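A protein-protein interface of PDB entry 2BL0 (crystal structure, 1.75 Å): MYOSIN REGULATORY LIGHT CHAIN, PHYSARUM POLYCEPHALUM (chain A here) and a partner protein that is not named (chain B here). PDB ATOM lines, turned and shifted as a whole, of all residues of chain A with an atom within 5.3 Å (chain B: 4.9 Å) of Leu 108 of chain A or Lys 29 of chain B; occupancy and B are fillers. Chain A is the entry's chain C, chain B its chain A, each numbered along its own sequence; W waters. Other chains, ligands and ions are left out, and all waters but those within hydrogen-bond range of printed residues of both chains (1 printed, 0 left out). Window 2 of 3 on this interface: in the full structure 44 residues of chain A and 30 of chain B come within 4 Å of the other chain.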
ATOM      1  N   THR A  87      13.821  -9.914  11.384  1.00  0.00           N
ATOM      2  CA  THR A  87      14.807 -10.693  10.655  1.00  0.00           C
ATOM      3  C   THR A  87      15.715 -11.435  11.627  1.00  0.00           C
ATOM      4  O   THR A  87      16.063 -12.587  11.398  1.00  0.00           O
ATOM      5  CB  THR A  87      15.630  -9.759   9.754  1.00  0.00           C
ATOM      6  OG1 THR A  87      14.769  -9.165   8.776  1.00  0.00           O
ATOM      7  CG2 THR A  87      16.676 -10.532   8.935  1.00  0.00           C
ATOM      8  N   PHE A  88      16.073 -10.760  12.719  1.00  0.00           N
ATOM      9  CA  PHE A  88      16.956 -11.293  13.752  1.00  0.00           C
ATOM     10  C   PHE A  88      16.211 -11.864  14.962  1.00  0.00           C
ATOM     11  O   PHE A  88      16.828 -12.249  15.955  1.00  0.00           O
ATOM     12  CB  PHE A  88      17.918 -10.197  14.189  1.00  0.00           C
ATOM     13  CG  PHE A  88      18.680  -9.608  13.045  1.00  0.00           C
ATOM     14  CD1 PHE A  88      18.240  -8.444  12.421  1.00  0.00           C
ATOM     15  CD2 PHE A  88      19.812 -10.241  12.562  1.00  0.00           C
ATOM     16  CE1 PHE A  88      18.931  -7.918  11.345  1.00  0.00           C
ATOM     17  CE2 PHE A  88      20.515  -9.718  11.489  1.00  0.00           C
ATOM     18  CZ  PHE A  88      20.076  -8.564  10.873  1.00  0.00           C
ATOM     19  N   ALA A 100      24.595 -11.977  18.436  1.00  0.00           N
ATOM     20  CA  ALA A 100      24.032 -12.113  17.083  1.00  0.00           C
ATOM     21  C   ALA A 100      23.775 -10.782  16.357  1.00  0.00           C
ATOM     22  O   ALA A 100      24.129 -10.650  15.175  1.00  0.00           O
ATOM     23  CB  ALA A 100      22.738 -12.904  17.140  1.00  0.00           C
ATOM     24  N   ASP A 103      27.297  -8.780  15.794  1.00  0.00           N
ATOM     25  CA  ASP A 103      28.041  -9.098  14.580  1.00  0.00           C
ATOM     26  C   ASP A 103      27.281  -8.532  13.347  1.00  0.00           C
ATOM     27  O   ASP A 103      27.896  -7.935  12.466  1.00  0.00           O
ATOM     28  CB  ASP A 103      28.546 -10.571  14.497  1.00  0.00           C
ATOM     29  CG  ASP A 103      27.446 -11.640  14.604  1.00  0.00           C
ATOM     30  OD1 ASP A 103      26.340 -11.464  13.984  1.00  0.00           O
ATOM     31  OD2 ASP A 103      27.654 -12.757  15.293  1.00  0.00           O
ATOM     32  N   ALA A 104      25.950  -8.581  13.352  1.00  0.00           N
ATOM     33  CA  ALA A 104      25.160  -8.030  12.236  1.00  0.00           C
ATOM     34  C   ALA A 104      25.267  -6.507  12.089  1.00  0.00           C
ATOM     35  O   ALA A 104      25.584  -5.998  11.026  1.00  0.00           O
ATOM     36  CB  ALA A 104      23.699  -8.416  12.376  1.00  0.00           C
ATOM     37  N   LEU A 105      24.994  -5.776  13.160  1.00  0.00           N
ATOM     38  CA  LEU A 105      24.939  -4.303  13.065  1.00  0.00           C
ATOM     39  C   LEU A 105      26.332  -3.677  12.945  1.00  0.00           C
ATOM     40  O   LEU A 105      26.469  -2.550  12.494  1.00  0.00           O
ATOM     41  CB  LEU A 105      24.221  -3.720  14.282  1.00  0.00           C
ATOM     42  CG  LEU A 105      22.766  -4.151  14.450  1.00  0.00           C
ATOM     43  CD1 LEU A 105      22.081  -3.293  15.525  1.00  0.00           C
ATOM     44  CD2 LEU A 105      21.999  -4.062  13.137  1.00  0.00           C
ATOM     45  N   LEU A 106      27.356  -4.397  13.393  1.00  0.00           N
ATOM     46  CA  LEU A 106      28.737  -3.895  13.353  1.00  0.00           C
ATOM     47  C   LEU A 106      29.466  -4.286  12.073  1.00  0.00           C
ATOM     48  O   LEU A 106      30.473  -3.683  11.734  1.00  0.00           O
ATOM     49  CB  LEU A 106      29.542  -4.383  14.568  1.00  0.00           C
ATOM     50  CG  LEU A 106      29.334  -3.604  15.884  1.00  0.00           C
ATOM     51  CD1 LEU A 106      30.020  -2.244  15.824  1.00  0.00           C
ATOM     52  CD2 LEU A 106      27.856  -3.396  16.261  1.00  0.00           C
ATOM     53  N   ASN A 107      28.989  -5.307  11.376  1.00  0.00           N
ATOM     54  CA  ASN A 107      29.734  -5.824  10.216  1.00  0.00           C
ATOM     55  C   ASN A 107      29.027  -5.634   8.870  1.00  0.00           C
ATOM     56  O   ASN A 107      29.689  -5.555   7.823  1.00  0.00           O
ATOM     57  CB  ASN A 107      30.084  -7.315  10.395  1.00  0.00           C
ATOM     58  CG  ASN A 107      30.915  -7.608  11.665  1.00  0.00           C
ATOM     59  OD1 ASN A 107      30.913  -8.741  12.154  1.00  0.00           O
ATOM     60  ND2 ASN A 107      31.647  -6.619  12.163  1.00  0.00           N
ATOM     61  N   LEU A 108      27.695  -5.605   8.894  1.00  0.00           N
ATOM     62  CA  LEU A 108      26.872  -5.520   7.682  1.00  0.00           C
ATOM     63  C   LEU A 108      26.414  -4.092   7.421  1.00  0.00           C
ATOM     64  O   LEU A 108      26.499  -3.226   8.288  1.00  0.00           O
ATOM     65  CB  LEU A 108      25.623  -6.412   7.794  1.00  0.00           C
ATOM     66  CG  LEU A 108      25.617  -7.896   7.403  1.00  0.00           C
ATOM     67  CD1 LEU A 108      27.012  -8.534   7.265  1.00  0.00           C
ATOM     68  CD2 LEU A 108      24.784  -8.647   8.390  1.00  0.00           C
ATOM     69  N   GLY A 109      25.909  -3.855   6.213  1.00  0.00           N
ATOM     70  CA  GLY A 109      25.273  -2.590   5.895  1.00  0.00           C
ATOM     71  C   GLY A 109      26.197  -1.407   6.118  1.00  0.00           C
ATOM     72  O   GLY A 109      27.391  -1.469   5.802  1.00  0.00           O
ATOM     73  N   ASP A 110      25.632  -0.317   6.632  1.00  0.00           N
ATOM     74  CA  ASP A 110      26.412   0.858   6.988  1.00  0.00           C
ATOM     75  C   ASP A 110      26.752   0.690   8.461  1.00  0.00           C
ATOM     76  O   ASP A 110      26.024   1.141   9.350  1.00  0.00           O
ATOM     77  CB  ASP A 110      25.618   2.145   6.706  1.00  0.00           C
ATOM     78  CG  ASP A 110      26.512   3.340   6.421  1.00  0.00           C
ATOM     79  OD1 ASP A 110      27.741   3.254   6.652  1.00  0.00           O
ATOM     80  OD2 ASP A 110      26.061   4.421   5.963  1.00  0.00           O
ATOM     81  N   ARG A 111      27.860  -0.003   8.699  1.00  0.00           N
ATOM     82  CA  ARG A 111      28.206  -0.477  10.036  1.00  0.00           C
ATOM     83  C   ARG A 111      28.201   0.609  11.113  1.00  0.00           C
ATOM     84  O   ARG A 111      28.739   1.716  10.948  1.00  0.00           O
ATOM     85  CB  ARG A 111      29.555  -1.198  10.041  1.00  0.00           C
ATOM     86  CG  ARG A 111      30.771  -0.337   9.710  1.00  0.00           C
ATOM     87  CD  ARG A 111      32.084  -1.113   9.722  1.00  0.00           C
ATOM     88  NE  ARG A 111      32.116  -2.197   8.735  1.00  0.00           N
ATOM     89  CZ  ARG A 111      33.017  -3.182   8.731  1.00  0.00           C
ATOM     90  NH1 ARG A 111      32.970  -4.125   7.791  1.00  0.00           N
ATOM     91  NH2 ARG A 111      33.968  -3.233   9.667  1.00  0.00           N
ATOM     92  N   GLN B  25      18.974 -14.851   1.518  1.00  0.00           N
ATOM     93  CA  GLN B  25      19.245 -14.820   2.959  1.00  0.00           C
ATOM     94  C   GLN B  25      20.176 -13.672   3.336  1.00  0.00           C
ATOM     95  O   GLN B  25      19.897 -12.920   4.285  1.00  0.00           O
ATOM     96  CB  GLN B  25      19.863 -16.153   3.430  1.00  0.00           C
ATOM     97  CG  GLN B  25      20.736 -16.085   4.714  1.00  0.00           C
ATOM     98  CD  GLN B  25      22.225 -15.792   4.456  1.00  0.00           C
ATOM     99  OE1 GLN B  25      22.870 -15.095   5.262  1.00  0.00           O
ATOM    100  NE2 GLN B  25      22.769 -16.314   3.346  1.00  0.00           N
ATOM    101  N   ALA B  26      21.285 -13.569   2.618  1.00  0.00           N
ATOM    102  CA  ALA B  26      22.304 -12.571   2.908  1.00  0.00           C
ATOM    103  C   ALA B  26      21.773 -11.163   2.699  1.00  0.00           C
ATOM    104  O   ALA B  26      22.077 -10.264   3.477  1.00  0.00           O
ATOM    105  CB  ALA B  26      23.512 -12.793   2.051  1.00  0.00           C
ATOM    106  N   ARG B  27      20.986 -10.974   1.640  1.00  0.00           N
ATOM    107  CA  ARG B  27      20.379  -9.672   1.339  1.00  0.00           C
ATOM    108  C   ARG B  27      19.336  -9.291   2.385  1.00  0.00           C
ATOM    109  O   ARG B  27      19.285  -8.148   2.815  1.00  0.00           O
ATOM    110  CB  ARG B  27      19.726  -9.663  -0.048  1.00  0.00           C
ATOM    111  CG  ARG B  27      19.278  -8.288  -0.458  1.00  0.00           C
ATOM    112  CD  ARG B  27      18.563  -8.180  -1.798  1.00  0.00           C
ATOM    113  NE  ARG B  27      17.683  -7.008  -1.771  1.00  0.00           N
ATOM    114  CZ  ARG B  27      16.506  -6.975  -1.155  1.00  0.00           C
ATOM    115  NH1 ARG B  27      16.032  -8.052  -0.540  1.00  0.00           N
ATOM    116  NH2 ARG B  27      15.789  -5.864  -1.174  1.00  0.00           N
ATOM    117  N   GLU B  28      18.527 -10.251   2.816  1.00  0.00           N
ATOM    118  CA  GLU B  28      17.499  -9.951   3.813  1.00  0.00           C
ATOM    119  C   GLU B  28      18.161  -9.458   5.083  1.00  0.00           C
ATOM    120  O   GLU B  28      17.738  -8.449   5.657  1.00  0.00           O
ATOM    121  CB  GLU B  28      16.590 -11.162   4.067  1.00  0.00           C
ATOM    122  CG  GLU B  28      15.516 -11.348   2.981  1.00  0.00           C
ATOM    123  CD  GLU B  28      14.764 -12.675   3.048  1.00  0.00           C
ATOM    124  OE1 GLU B  28      15.186 -13.601   3.781  1.00  0.00           O
ATOM    125  OE2 GLU B  28      13.744 -12.807   2.330  1.00  0.00           O
ATOM    126  N   LYS B  29      19.231 -10.136   5.494  1.00  0.00           N
ATOM    127  CA  LYS B  29      19.996  -9.756   6.678  1.00  0.00           C
ATOM    128  C   LYS B  29      20.620  -8.378   6.519  1.00  0.00           C
ATOM    129  O   LYS B  29      20.552  -7.566   7.445  1.00  0.00           O
ATOM    130  CB  LYS B  29      21.076 -10.809   6.981  1.00  0.00           C
ATOM    131  CG  LYS B  29      21.816 -10.636   8.279  1.00  0.00           C
ATOM    132  CD  LYS B  29      22.784 -11.801   8.564  1.00  0.00           C
ATOM    133  CE  LYS B  29      23.327 -11.787  10.001  1.00  0.00           C
ATOM    134  NZ  LYS B  29      24.800 -11.629  10.135  1.00  0.00           N
ATOM    135  N   SER B  30      21.211  -8.093   5.354  1.00  0.00           N
ATOM    136  CA  SER B  30      21.885  -6.803   5.155  1.00  0.00           C
ATOM    137  C   SER B  30      20.896  -5.637   5.077  1.00  0.00           C
ATOM    138  O   SER B  30      21.169  -4.541   5.586  1.00  0.00           O
ATOM    139  CB  SER B  30      22.770  -6.802   3.900  1.00  0.00           C
ATOM    140  OG  SER B  30      24.049  -7.379   4.201  1.00  0.00           O
ATOM    141  N   VAL B  31      19.753  -5.868   4.441  1.00  0.00           N
ATOM    142  CA  VAL B  31      18.738  -4.823   4.287  1.00  0.00           C
ATOM    143  C   VAL B  31      18.151  -4.479   5.657  1.00  0.00           C
ATOM    144  O   VAL B  31      17.963  -3.301   5.985  1.00  0.00           O
ATOM    145  CB  VAL B  31      17.628  -5.255   3.282  1.00  0.00           C
ATOM    146  CG1 VAL B  31      16.340  -4.429   3.447  1.00  0.00           C
ATOM    147  CG2 VAL B  31      18.140  -5.143   1.855  1.00  0.00           C
ATOM    148  N   SER B  32      17.883  -5.504   6.450  1.00  0.00           N
ATOM    149  CA  SER B  32      17.339  -5.326   7.801  1.00  0.00           C
ATOM    150  C   SER B  32      18.325  -4.637   8.726  1.00  0.00           C
ATOM    151  O   SER B  32      17.940  -3.755   9.487  1.00  0.00           O
ATOM    152  CB  SER B  32      16.903  -6.657   8.386  1.00  0.00           C
ATOM    153  OG  SER B  32      15.749  -7.123   7.722  1.00  0.00           O
ATOM    154  N   ALA B  33      19.590  -5.036   8.659  1.00  0.00           N
ATOM    155  CA  ALA B  33      20.642  -4.416   9.441  1.00  0.00           C
ATOM    156  C   ALA B  33      20.725  -2.951   9.076  1.00  0.00           C
ATOM    157  O   ALA B  33      20.857  -2.111   9.934  1.00  0.00           O
ATOM    158  CB  ALA B  33      21.965  -5.070   9.176  1.00  0.00           C
ATOM    159  N   GLN B  37      20.407   0.231  11.607  1.00  0.00           N
ATOM    160  CA  GLN B  37      21.517   1.168  11.695  1.00  0.00           C
ATOM    161  C   GLN B  37      21.057   2.598  11.417  1.00  0.00           C
ATOM    162  O   GLN B  37      21.400   3.525  12.150  1.00  0.00           O
ATOM    163  CB  GLN B  37      22.619   0.767  10.696  1.00  0.00           C
ATOM    164  CG  GLN B  37      23.305  -0.555  11.043  1.00  0.00           C
ATOM    165  CD  GLN B  37      23.978  -1.227   9.857  1.00  0.00           C
ATOM    166  OE1 GLN B  37      23.660  -0.934   8.697  1.00  0.00           O
ATOM    167  NE2 GLN B  37      24.907  -2.146  10.143  1.00  0.00           N
HETATM  168  O   HOH W   1      26.059  -5.824   4.065  1.00  0.00           O
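OG1 of Thr 87 of chain A sits at hydrogen-bond distance from OG of Ser 32 of chain B, at 2.5 Å. The side-chain amide nitrogen (NE2) of Gln 37 of chain B is in hydrogen-bond range of the backbone carbonyl oxygen (O) of Leu 105 of chain A, at 2.9 Å. The side-chain amide nitrogen (NE2) of Gln 37 of chain B sits at hydrogen-bond distance from the backbone carbonyl oxygen (O) of Leu 108 of chain A (2.7 Å). The side-chain amide oxygen (OE1) of Gln 37 of chain B lies within hydrogen-bond range of the backbone NH (N) of Asp 110 of chain A (2.9 Å).
O of Glu 28 of chain B sits at hydrogen-bond distance from OG of Ser 32 of chain B, at 3.2 Å. O of Ala 33 of chain B lies close to OE1 of Gln 37 of chain B, at 3.3 Å.
Among the printed residues, pairs that only touch across the chains: Leu 108 of chain A with Lys 29 of chain B (3.5 Å), Phe 88 of chain A with Lys 29 of chain B (3.6 Å), Leu 108 of chain A with Ser 30 of chain B (3.6 Å), Gly 109 of chain A with Gln 37 of chain B (3.6 Å), Arg 111 of chain A with Gln 37 of chain B (3.7 Å), Phe 88 of chain A with Ser 32 of chain B (3.8 Å), Leu 105 of chain A with Ala 33 of chain B (3.9 Å) and Phe 88 of chain A with Ala 33 of chain B (3.99 Å).
Leu 108 of chain A touches just these residues of chain B: Lys 29, Ser 30 and Gln 37. Printed residues of chain A within 4 Å of Lys 29 of chain B: Phe 88 (3.6 Å) and Leu 108 (3.5 Å). Printed residues of chain A within 4 Å of Ala 33 of chain B: Phe 88 (3.99 Å) and Leu 105 (3.9 Å). Printed residues of chain B within 4 Å of Leu 105 of chain A: Ala 33 and Gln 37. Of the printed residues of chain A, Ser 30 of chain B touches Leu 108 (3.6 Å). Of the printed residues of chain A, Gln 37 of chain B touches Leu 105 (2.9 Å), Leu 108 (2.7 Å), Gly 109 (3.6 Å), Asp 110 (2.9 Å) and Arg 111 (3.7 Å). The nearest residue of chain B that does not touch Leu 108 of chain A is Ala 33 of chain B (4.1 Å). The nearest printed residue of chain A that does not touch Lys 29 of chain B is Ala 104 of chain A (4.1 Å).
Of the 12 printed residues of chain A, 7 touch a printed residue of chain B. Printed residues of chain A that touch a printed residue of chain B: Thr 87, Phe 88, Leu 105, Leu 108, Gly 109, Asp 110 and Arg 111. Of the 10 printed residues of chain B, 5 touch a printed residue of chain A. Among the printed residues, no Asp or Glu carboxylate lies within 4 Å of a Lys or Arg side-chain nitrogen of the other chain.
Water W1 bridges the side-chain hydroxyl of Ser 30 of chain B (2.5 Å) and the backbone NH of Gly 109 of chain A (2.9 Å).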
